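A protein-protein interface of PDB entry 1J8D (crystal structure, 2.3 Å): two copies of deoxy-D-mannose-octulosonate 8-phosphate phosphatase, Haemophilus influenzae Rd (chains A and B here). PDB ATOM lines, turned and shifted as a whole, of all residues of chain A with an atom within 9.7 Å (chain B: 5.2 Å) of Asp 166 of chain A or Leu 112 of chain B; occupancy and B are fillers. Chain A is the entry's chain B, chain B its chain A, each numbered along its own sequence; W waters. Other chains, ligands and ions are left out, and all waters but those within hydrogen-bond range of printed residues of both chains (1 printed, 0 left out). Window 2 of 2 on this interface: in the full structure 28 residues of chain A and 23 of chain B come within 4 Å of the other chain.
The guanidinium group of Arg 149 of chain A lies within salt-bridge range of the side-chain carboxylate of Asp 108 of chain B (3.0 Å). The guanidinium group (NH2) of Arg 149 of chain A is in hydrogen-bond range of the side-chain hydroxyl (OG) of Ser 109 of chain B. The backbone carbonyl oxygen (O) of Phe 165 of chain A is in hydrogen-bond range of the side-chain hydroxyl (OG) of Ser 109 of chain B. NH2 of Arg 149 of chain A is in hydrogen-bond range of OH of Tyr 130 of chain B. OH of Tyr 130 of chain B is in hydrogen-bond range of OD1 of Asp 153 of chain A (2.5 Å).
The side-chain carboxylate (OD1) of Asp 108 of chain B lies within hydrogen-bond range of the side-chain hydroxyl (OG) of Ser 109 of chain B. The backbone NH (N) of Asp 108 of chain B is in hydrogen-bond range of the side-chain carboxylate (OD2) of Asp 111 of chain B (3.0 Å). The side-chain sulfur of Met 46 of chain A lies within hydrogen-bond range of the guanidinium group of Arg 149 of chain A (3.6 Å). The backbone carbonyl oxygen of Ser 163 of chain A sits at hydrogen-bond distance from the side-chain hydroxyl of Thr 167 of chain A (3.2 Å). The backbone carbonyl oxygen of Val 164 of chain A sits close to the backbone NH of Phe 171 of chain A (3.4 Å). The backbone NH (N) of Gly 170 of chain A lies within hydrogen-bond range of the side-chain hydroxyl (OG1) of Thr 167 of chain A.
Among the printed residues, pairs that only touch across the chains: Phe 165 of chain A with Tyr 130 of chain B (3.1 Å), Thr 167 of chain A with Leu 112 of chain B (3.3 Å), Leu 42 of chain A with Asp 108 of chain B (3.4 Å), Phe 171 of chain A with Val 110 of chain B (3.4 Å), Ala 168 of chain A with Leu 112 of chain B (3.5 Å), Leu 42 of chain A with Val 110 of chain B (3.7 Å), Asp 166 of chain A with Leu 112 of chain B (3.7 Å), Met 46 of chain A with Ser 109 of chain B (3.9 Å), Phe 165 of chain A with Leu 112 of chain B (3.9 Å) and Leu 172 of chain A with Pro 113 of chain B (3.9 Å).
Of the printed residues of chain B, Arg 149 of chain A touches Asp 108, Ser 109 and Tyr 130. Leu 156 of chain A touches none of the printed residues of chain B. Asp 166 of chain A touches just one residue of chain B: Leu 112. Of the printed residues of chain B, Phe 171 of chain A touches Val 110. Of the printed residues of chain B, Leu 172 of chain A touches Pro 113. No residue of chain A comes within 4 Å of Asp 111 of chain B. Of chain A, only Phe 165 (3.9 Å), Asp 166 (3.7 Å), Thr 167 (3.3 Å) and Ala 168 (3.5 Å) come within 4 Å of Leu 112 of chain B. Of chain A, only Leu 172 comes within 4 Å of Pro 113 of chain B. No residue of chain A comes within 4 Å of Ala 114 of chain B. No residue of chain A comes within 4 Å of Phe 115 of chain B. Of the printed residues of chain A, Tyr 130 of chain B touches Arg 149, Asp 153 and Phe 165. The nearest residue of chain B that does not touch Asp 166 of chain A is Tyr 130 of chain B (4.2 Å). The nearest residue of chain A that does not touch Leu 112 of chain B is Phe 171 of chain A (5.2 Å).
Hydrophobic or aromatic side chains of chain A within 4 Å of the printed part of chain B: Leu 42, Met 46, Phe 165, Ala 168, Phe 171 and Leu 172. Of the 12 printed residues of chain B, 6 touch a printed residue of chain A. Hydrophobic or aromatic side chains of chain B that line the printed part of chain A: Val 110, Leu 112, Pro 113 and Tyr 130.
No position is printed for both chains.
Water W1 bridges the backbone carbonyl oxygen (O) of Tyr 130 of chain B (2.7 Å) and the backbone carbonyl oxygen (O) of Asp 166 of chain A (3.2 Å).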
ATOM      1  N   LEU A  42      18.015  10.940  36.064  1.00  0.00           N
ATOM      2  CA  LEU A  42      18.547  10.475  34.811  1.00  0.00           C
ATOM      3  C   LEU A  42      18.819  11.650  33.847  1.00  0.00           C
ATOM      4  O   LEU A  42      19.801  11.651  33.100  1.00  0.00           O
ATOM      5  CB  LEU A  42      17.576   9.475  34.187  1.00  0.00           C
ATOM      6  CG  LEU A  42      18.097   8.686  32.980  1.00  0.00           C
ATOM      7  CD1 LEU A  42      19.240   7.783  33.415  1.00  0.00           C
ATOM      8  CD2 LEU A  42      16.989   7.870  32.401  1.00  0.00           C
ATOM      9  N   MET A  46      22.206  12.258  31.674  1.00  0.00           N
ATOM     10  CA  MET A  46      22.259  12.312  30.220  1.00  0.00           C
ATOM     11  C   MET A  46      22.942  13.609  29.807  1.00  0.00           C
ATOM     12  O   MET A  46      23.700  13.627  28.828  1.00  0.00           O
ATOM     13  CB  MET A  46      20.862  12.229  29.644  1.00  0.00           C
ATOM     14  CG  MET A  46      20.173  10.965  30.009  1.00  0.00           C
ATOM     15  SD  MET A  46      18.301  11.050  29.647  1.00  0.00           S
ATOM     16  CE  MET A  46      18.128   9.207  29.202  1.00  0.00           C
ATOM     17  N   ARG A 149      14.046  17.085  34.130  1.00  0.00           N
ATOM     18  CA  ARG A 149      14.112  16.121  33.043  1.00  0.00           C
ATOM     19  C   ARG A 149      13.471  16.673  31.773  1.00  0.00           C
ATOM     20  O   ARG A 149      13.980  16.488  30.669  1.00  0.00           O
ATOM     21  CB  ARG A 149      13.441  14.803  33.458  1.00  0.00           C
ATOM     22  CG  ARG A 149      13.401  13.770  32.349  1.00  0.00           C
ATOM     23  CD  ARG A 149      14.758  13.641  31.706  1.00  0.00           C
ATOM     24  NE  ARG A 149      14.828  12.526  30.777  1.00  0.00           N
ATOM     25  CZ  ARG A 149      14.777  11.244  31.129  1.00  0.00           C
ATOM     26  NH1 ARG A 149      14.668  10.896  32.402  1.00  0.00           N
ATOM     27  NH2 ARG A 149      14.796  10.311  30.192  1.00  0.00           N
ATOM     28  N   ASP A 153      15.660  17.024  28.460  1.00  0.00           N
ATOM     29  CA  ASP A 153      15.304  16.417  27.184  1.00  0.00           C
ATOM     30  C   ASP A 153      15.319  17.501  26.076  1.00  0.00           C
ATOM     31  O   ASP A 153      15.897  17.288  25.007  1.00  0.00           O
ATOM     32  CB  ASP A 153      13.937  15.746  27.272  1.00  0.00           C
ATOM     33  CG  ASP A 153      13.965  14.421  28.050  1.00  0.00           C
ATOM     34  OD1 ASP A 153      12.866  13.969  28.428  1.00  0.00           O
ATOM     35  OD2 ASP A 153      15.048  13.816  28.272  1.00  0.00           O
ATOM     36  N   MET A 154      14.709  18.657  26.328  1.00  0.00           N
ATOM     37  CA  MET A 154      14.705  19.739  25.336  1.00  0.00           C
ATOM     38  C   MET A 154      16.108  20.085  24.851  1.00  0.00           C
ATOM     39  O   MET A 154      16.370  20.150  23.650  1.00  0.00           O
ATOM     40  CB  MET A 154      14.113  20.999  25.912  1.00  0.00           C
ATOM     41  CG  MET A 154      12.634  20.985  26.024  1.00  0.00           C
ATOM     42  SD  MET A 154      12.138  22.612  26.898  1.00  0.00           S
ATOM     43  CE  MET A 154      10.959  21.876  28.213  1.00  0.00           C
ATOM     44  N   LEU A 156      19.155  18.369  25.077  1.00  0.00           N
ATOM     45  CA  LEU A 156      19.704  17.261  24.298  1.00  0.00           C
ATOM     46  C   LEU A 156      19.031  17.137  22.950  1.00  0.00           C
ATOM     47  O   LEU A 156      19.689  16.920  21.945  1.00  0.00           O
ATOM     48  CB  LEU A 156      19.566  15.938  25.063  1.00  0.00           C
ATOM     49  CG  LEU A 156      20.507  15.913  26.257  1.00  0.00           C
ATOM     50  CD1 LEU A 156      20.322  14.619  27.062  1.00  0.00           C
ATOM     51  CD2 LEU A 156      21.935  16.051  25.732  1.00  0.00           C
ATOM     52  N   GLN A 157      17.717  17.292  22.934  1.00  0.00           N
ATOM     53  CA  GLN A 157      16.978  17.179  21.696  1.00  0.00           C
ATOM     54  C   GLN A 157      17.558  18.204  20.729  1.00  0.00           C
ATOM     55  O   GLN A 157      18.120  17.844  19.701  1.00  0.00           O
ATOM     56  CB  GLN A 157      15.506  17.455  21.953  1.00  0.00           C
ATOM     57  CG  GLN A 157      14.623  17.198  20.768  1.00  0.00           C
ATOM     58  CD  GLN A 157      14.483  15.721  20.481  1.00  0.00           C
ATOM     59  OE1 GLN A 157      13.819  14.992  21.225  1.00  0.00           O
ATOM     60  NE2 GLN A 157      15.125  15.259  19.403  1.00  0.00           N
ATOM     61  N   ALA A 158      17.440  19.480  21.097  1.00  0.00           N
ATOM     62  CA  ALA A 158      17.933  20.597  20.299  1.00  0.00           C
ATOM     63  C   ALA A 158      19.370  20.401  19.792  1.00  0.00           C
ATOM     64  O   ALA A 158      19.753  20.947  18.749  1.00  0.00           O
ATOM     65  CB  ALA A 158      17.838  21.887  21.112  1.00  0.00           C
ATOM     66  N   GLY A 160      20.641  17.417  19.016  1.00  0.00           N
ATOM     67  CA  GLY A 160      20.752  16.205  18.231  1.00  0.00           C
ATOM     68  C   GLY A 160      21.353  15.073  19.024  1.00  0.00           C
ATOM     69  O   GLY A 160      22.118  14.266  18.492  1.00  0.00           O
ATOM     70  N   LYS A 161      21.003  14.996  20.306  1.00  0.00           N
ATOM     71  CA  LYS A 161      21.532  13.937  21.153  1.00  0.00           C
ATOM     72  C   LYS A 161      20.416  13.139  21.840  1.00  0.00           C
ATOM     73  O   LYS A 161      20.665  12.320  22.708  1.00  0.00           O
ATOM     74  CB  LYS A 161      22.494  14.547  22.173  1.00  0.00           C
ATOM     75  CG  LYS A 161      23.672  15.232  21.508  1.00  0.00           C
ATOM     76  CD  LYS A 161      24.672  15.838  22.495  1.00  0.00           C
ATOM     77  CE  LYS A 161      25.768  16.636  21.749  1.00  0.00           C
ATOM     78  NZ  LYS A 161      27.011  16.863  22.567  1.00  0.00           N
ATOM     79  N   SER A 162      19.184  13.361  21.409  1.00  0.00           N
ATOM     80  CA  SER A 162      18.047  12.685  22.006  1.00  0.00           C
ATOM     81  C   SER A 162      18.172  11.177  21.997  1.00  0.00           C
ATOM     82  O   SER A 162      17.482  10.493  22.757  1.00  0.00           O
ATOM     83  CB  SER A 162      16.755  13.086  21.298  1.00  0.00           C
ATOM     84  OG  SER A 162      16.653  12.449  20.032  1.00  0.00           O
ATOM     85  N   SER A 163      19.044  10.645  21.156  1.00  0.00           N
ATOM     86  CA  SER A 163      19.195   9.189  21.094  1.00  0.00           C
ATOM     87  C   SER A 163      19.381   8.499  22.450  1.00  0.00           C
ATOM     88  O   SER A 163      18.892   7.384  22.617  1.00  0.00           O
ATOM     89  CB  SER A 163      20.337   8.789  20.142  1.00  0.00           C
ATOM     90  OG  SER A 163      21.342   9.789  20.083  1.00  0.00           O
ATOM     91  N   VAL A 164      20.058   9.153  23.409  1.00  0.00           N
ATOM     92  CA  VAL A 164      20.261   8.554  24.742  1.00  0.00           C
ATOM     93  C   VAL A 164      18.960   8.283  25.482  1.00  0.00           C
ATOM     94  O   VAL A 164      18.830   7.246  26.147  1.00  0.00           O
ATOM     95  CB  VAL A 164      21.133   9.408  25.676  1.00  0.00           C
ATOM     96  CG1 VAL A 164      22.582   9.276  25.279  1.00  0.00           C
ATOM     97  CG2 VAL A 164      20.673  10.845  25.647  1.00  0.00           C
ATOM     98  N   PHE A 165      18.000   9.195  25.391  1.00  0.00           N
ATOM     99  CA  PHE A 165      16.726   8.946  26.049  1.00  0.00           C
ATOM    100  C   PHE A 165      15.658   8.477  25.051  1.00  0.00           C
ATOM    101  O   PHE A 165      14.643   7.927  25.433  1.00  0.00           O
ATOM    102  CB  PHE A 165      16.253  10.195  26.805  1.00  0.00           C
ATOM    103  CG  PHE A 165      15.972  11.373  25.935  1.00  0.00           C
ATOM    104  CD1 PHE A 165      14.849  11.405  25.112  1.00  0.00           C
ATOM    105  CD2 PHE A 165      16.817  12.477  25.947  1.00  0.00           C
ATOM    106  CE1 PHE A 165      14.572  12.520  24.312  1.00  0.00           C
ATOM    107  CE2 PHE A 165      16.544  13.596  25.152  1.00  0.00           C
ATOM    108  CZ  PHE A 165      15.417  13.613  24.335  1.00  0.00           C
ATOM    109  N   ASP A 166      15.945   8.670  23.769  1.00  0.00           N
ATOM    110  CA  ASP A 166      15.038   8.360  22.657  1.00  0.00           C
ATOM    111  C   ASP A 166      14.888   6.904  22.261  1.00  0.00           C
ATOM    112  O   ASP A 166      13.792   6.452  21.942  1.00  0.00           O
ATOM    113  CB  ASP A 166      15.516   9.111  21.408  1.00  0.00           C
ATOM    114  CG  ASP A 166      14.416   9.812  20.720  1.00  0.00           C
ATOM    115  OD1 ASP A 166      13.374   9.162  20.485  1.00  0.00           O
ATOM    116  OD2 ASP A 166      14.588  11.007  20.414  1.00  0.00           O
ATOM    117  N   THR A 167      16.006   6.194  22.238  1.00  0.00           N
ATOM    118  CA  THR A 167      16.012   4.806  21.821  1.00  0.00           C
ATOM    119  C   THR A 167      16.744   3.886  22.758  1.00  0.00           C
ATOM    120  O   THR A 167      17.576   4.309  23.569  1.00  0.00           O
ATOM    121  CB  THR A 167      16.674   4.642  20.428  1.00  0.00           C
ATOM    122  OG1 THR A 167      18.009   5.154  20.461  1.00  0.00           O
ATOM    123  CG2 THR A 167      15.893   5.397  19.382  1.00  0.00           C
ATOM    124  N   ALA A 168      16.420   2.611  22.629  1.00  0.00           N
ATOM    125  CA  ALA A 168      17.047   1.595  23.421  1.00  0.00           C
ATOM    126  C   ALA A 168      18.524   1.671  23.100  1.00  0.00           C
ATOM    127  O   ALA A 168      19.346   1.817  23.994  1.00  0.00           O
ATOM    128  CB  ALA A 168      16.505   0.243  23.050  1.00  0.00           C
ATOM    129  N   GLN A 169      18.879   1.613  21.821  1.00  0.00           N
ATOM    130  CA  GLN A 169      20.299   1.639  21.499  1.00  0.00           C
ATOM    131  C   GLN A 169      21.056   2.838  22.097  1.00  0.00           C
ATOM    132  O   GLN A 169      22.082   2.661  22.764  1.00  0.00           O
ATOM    133  CB  GLN A 169      20.517   1.563  19.985  1.00  0.00           C
ATOM    134  CG  GLN A 169      21.986   1.338  19.637  1.00  0.00           C
ATOM    135  CD  GLN A 169      22.201   0.672  18.283  1.00  0.00           C
ATOM    136  OE1 GLN A 169      21.984  -0.536  18.124  1.00  0.00           O
ATOM    137  NE2 GLN A 169      22.626   1.459  17.303  1.00  0.00           N
ATOM    138  N   GLY A 170      20.557   4.051  21.857  1.00  0.00           N
ATOM    139  CA  GLY A 170      21.211   5.222  22.410  1.00  0.00           C
ATOM    140  C   GLY A 170      21.352   5.067  23.920  1.00  0.00           C
ATOM    141  O   GLY A 170      22.407   5.368  24.482  1.00  0.00           O
ATOM    142  N   PHE A 171      20.317   4.561  24.587  1.00  0.00           N
ATOM    143  CA  PHE A 171      20.419   4.404  26.037  1.00  0.00           C
ATOM    144  C   PHE A 171      21.542   3.471  26.436  1.00  0.00           C
ATOM    145  O   PHE A 171      22.432   3.865  27.186  1.00  0.00           O
ATOM    146  CB  PHE A 171      19.112   3.895  26.661  1.00  0.00           C
ATOM    147  CG  PHE A 171      19.132   3.911  28.173  1.00  0.00           C
ATOM    148  CD1 PHE A 171      19.104   5.121  28.868  1.00  0.00           C
ATOM    149  CD2 PHE A 171      19.279   2.735  28.891  1.00  0.00           C
ATOM    150  CE1 PHE A 171      19.233   5.166  30.252  1.00  0.00           C
ATOM    151  CE2 PHE A 171      19.407   2.768  30.293  1.00  0.00           C
ATOM    152  CZ  PHE A 171      19.386   3.998  30.971  1.00  0.00           C
ATOM    153  N   LEU A 172      21.504   2.233  25.950  1.00  0.00           N
ATOM    154  CA  LEU A 172      22.547   1.266  26.276  1.00  0.00           C
ATOM    155  C   LEU A 172      23.934   1.842  26.024  1.00  0.00           C
ATOM    156  O   LEU A 172      24.828   1.694  26.861  1.00  0.00           O
ATOM    157  CB  LEU A 172      22.377  -0.022  25.455  1.00  0.00           C
ATOM    158  CG  LEU A 172      21.373  -1.113  25.883  1.00  0.00           C
ATOM    159  CD1 LEU A 172      19.920  -0.607  25.852  1.00  0.00           C
ATOM    160  CD2 LEU A 172      21.548  -2.302  24.931  1.00  0.00           C
ATOM    161  N   MET A 178      24.537   6.496  33.455  1.00  0.00           N
ATOM    162  CA  MET A 178      23.160   6.846  33.804  1.00  0.00           C
ATOM    163  C   MET A 178      22.788   6.700  35.287  1.00  0.00           C
ATOM    164  O   MET A 178      21.690   7.091  35.727  1.00  0.00           O
ATOM    165  CB  MET A 178      22.222   5.997  32.948  1.00  0.00           C
ATOM    166  CG  MET A 178      22.422   6.194  31.444  1.00  0.00           C
ATOM    167  SD  MET A 178      22.018   8.002  30.848  1.00  0.00           S
ATOM    168  CE  MET A 178      23.760   8.807  30.882  1.00  0.00           C
ATOM    169  N   ASP B 108      10.429   4.878  31.940  1.00  0.00           N
ATOM    170  CA  ASP B 108      11.479   5.741  31.401  1.00  0.00           C
ATOM    171  C   ASP B 108      12.368   5.088  30.339  1.00  0.00           C
ATOM    172  O   ASP B 108      12.261   3.888  30.045  1.00  0.00           O
ATOM    173  CB  ASP B 108      12.324   6.307  32.567  1.00  0.00           C
ATOM    174  CG  ASP B 108      12.987   7.645  32.233  1.00  0.00           C
ATOM    175  OD1 ASP B 108      12.803   8.146  31.103  1.00  0.00           O
ATOM    176  OD2 ASP B 108      13.695   8.199  33.100  1.00  0.00           O
ATOM    177  N   SER B 109      13.235   5.896  29.753  1.00  0.00           N
ATOM    178  CA  SER B 109      14.155   5.457  28.695  1.00  0.00           C
ATOM    179  C   SER B 109      14.794   4.143  29.064  1.00  0.00           C
ATOM    180  O   SER B 109      14.911   3.252  28.242  1.00  0.00           O
ATOM    181  CB  SER B 109      15.243   6.508  28.472  1.00  0.00           C
ATOM    182  OG  SER B 109      14.662   7.789  28.261  1.00  0.00           O
ATOM    183  N   VAL B 110      15.203   4.043  30.320  1.00  0.00           N
ATOM    184  CA  VAL B 110      15.826   2.840  30.865  1.00  0.00           C
ATOM    185  C   VAL B 110      15.033   1.570  30.541  1.00  0.00           C
ATOM    186  O   VAL B 110      15.610   0.500  30.429  1.00  0.00           O
ATOM    187  CB  VAL B 110      15.927   2.909  32.410  1.00  0.00           C
ATOM    188  CG1 VAL B 110      16.753   1.711  32.941  1.00  0.00           C
ATOM    189  CG2 VAL B 110      16.519   4.267  32.843  1.00  0.00           C
ATOM    190  N   ASP B 111      13.714   1.705  30.405  1.00  0.00           N
ATOM    191  CA  ASP B 111      12.835   0.570  30.135  1.00  0.00           C
ATOM    192  C   ASP B 111      12.671   0.211  28.656  1.00  0.00           C
ATOM    193  O   ASP B 111      12.119  -0.833  28.332  1.00  0.00           O
ATOM    194  CB  ASP B 111      11.463   0.857  30.739  1.00  0.00           C
ATOM    195  CG  ASP B 111      11.527   1.029  32.250  1.00  0.00           C
ATOM    196  OD1 ASP B 111      12.102   0.143  32.877  1.00  0.00           O
ATOM    197  OD2 ASP B 111      11.019   2.027  32.811  1.00  0.00           O
ATOM    198  N   LEU B 112      13.130   1.068  27.758  1.00  0.00           N
ATOM    199  CA  LEU B 112      12.981   0.787  26.338  1.00  0.00           C
ATOM    200  C   LEU B 112      13.458  -0.622  26.047  1.00  0.00           C
ATOM    201  O   LEU B 112      12.731  -1.423  25.493  1.00  0.00           O
ATOM    202  CB  LEU B 112      13.768   1.798  25.485  1.00  0.00           C
ATOM    203  CG  LEU B 112      13.307   3.249  25.631  1.00  0.00           C
ATOM    204  CD1 LEU B 112      14.211   4.126  24.817  1.00  0.00           C
ATOM    205  CD2 LEU B 112      11.830   3.412  25.186  1.00  0.00           C
ATOM    206  N   PRO B 113      14.689  -0.955  26.448  1.00  0.00           N
ATOM    207  CA  PRO B 113      15.140  -2.324  26.155  1.00  0.00           C
ATOM    208  C   PRO B 113      14.195  -3.418  26.647  1.00  0.00           C
ATOM    209  O   PRO B 113      14.038  -4.450  25.997  1.00  0.00           O
ATOM    210  CB  PRO B 113      16.533  -2.388  26.804  1.00  0.00           C
ATOM    211  CG  PRO B 113      16.506  -1.226  27.844  1.00  0.00           C
ATOM    212  CD  PRO B 113      15.728  -0.163  27.127  1.00  0.00           C
ATOM    213  N   ALA B 114      13.567  -3.178  27.793  1.00  0.00           N
ATOM    214  CA  ALA B 114      12.634  -4.131  28.388  1.00  0.00           C
ATOM    215  C   ALA B 114      11.415  -4.305  27.483  1.00  0.00           C
ATOM    216  O   ALA B 114      10.946  -5.426  27.214  1.00  0.00           O
ATOM    217  CB  ALA B 114      12.198  -3.641  29.726  1.00  0.00           C
ATOM    218  N   PHE B 115      10.885  -3.183  27.025  1.00  0.00           N
ATOM    219  CA  PHE B 115       9.736  -3.209  26.145  1.00  0.00           C
ATOM    220  C   PHE B 115       9.969  -4.132  24.951  1.00  0.00           C
ATOM    221  O   PHE B 115       9.105  -4.966  24.635  1.00  0.00           O
ATOM    222  CB  PHE B 115       9.442  -1.784  25.694  1.00  0.00           C
ATOM    223  CG  PHE B 115       9.088  -0.871  26.823  1.00  0.00           C
ATOM    224  CD1 PHE B 115       9.244   0.512  26.693  1.00  0.00           C
ATOM    225  CD2 PHE B 115       8.568  -1.391  28.022  1.00  0.00           C
ATOM    226  CE1 PHE B 115       8.879   1.379  27.745  1.00  0.00           C
ATOM    227  CE2 PHE B 115       8.196  -0.528  29.086  1.00  0.00           C
ATOM    228  CZ  PHE B 115       8.352   0.857  28.943  1.00  0.00           C
ATOM    229  N   ALA B 116      11.136  -3.998  24.315  1.00  0.00           N
ATOM    230  CA  ALA B 116      11.534  -4.799  23.143  1.00  0.00           C
ATOM    231  C   ALA B 116      11.720  -6.274  23.450  1.00  0.00           C
ATOM    232  O   ALA B 116      11.382  -7.129  22.636  1.00  0.00           O
ATOM    233  CB  ALA B 116      12.813  -4.249  22.546  1.00  0.00           C
ATOM    234  N   TYR B 130       8.297   9.400  24.478  1.00  0.00           N
ATOM    235  CA  TYR B 130       9.207   8.491  23.789  1.00  0.00           C
ATOM    236  C   TYR B 130       9.244   7.137  24.465  1.00  0.00           C
ATOM    237  O   TYR B 130       9.932   6.231  23.990  1.00  0.00           O
ATOM    238  CB  TYR B 130      10.614   9.090  23.663  1.00  0.00           C
ATOM    239  CG  TYR B 130      11.163   9.709  24.940  1.00  0.00           C
ATOM    240  CD1 TYR B 130      11.730   8.917  25.957  1.00  0.00           C
ATOM    241  CD2 TYR B 130      11.102  11.100  25.141  1.00  0.00           C
ATOM    242  CE1 TYR B 130      12.218   9.506  27.142  1.00  0.00           C
ATOM    243  CE2 TYR B 130      11.581  11.686  26.306  1.00  0.00           C
ATOM    244  CZ  TYR B 130      12.133  10.887  27.301  1.00  0.00           C
ATOM    245  OH  TYR B 130      12.560  11.486  28.458  1.00  0.00           O
ATOM    246  N   VAL B 131       8.504   7.014  25.572  1.00  0.00           N
ATOM    247  CA  VAL B 131       8.346   5.740  26.290  1.00  0.00           C
ATOM    248  C   VAL B 131       6.962   5.188  25.909  1.00  0.00           C
ATOM    249  O   VAL B 131       6.799   4.007  25.660  1.00  0.00           O
ATOM    250  CB  VAL B 131       8.346   5.906  27.838  1.00  0.00           C
ATOM    251  CG1 VAL B 131       7.702   4.664  28.496  1.00  0.00           C
ATOM    252  CG2 VAL B 131       9.752   6.132  28.345  1.00  0.00           C
ATOM    253  N   ALA B 134       7.019   3.468  22.661  1.00  0.00           N
ATOM    254  CA  ALA B 134       7.631   2.158  22.601  1.00  0.00           C
ATOM    255  C   ALA B 134       6.827   1.015  23.195  1.00  0.00           C
ATOM    256  O   ALA B 134       7.265  -0.138  23.125  1.00  0.00           O
ATOM    257  CB  ALA B 134       9.018   2.223  23.256  1.00  0.00           C
HETATM  258  O   HOH W   1      10.700   5.564  21.511  1.00  0.00           O
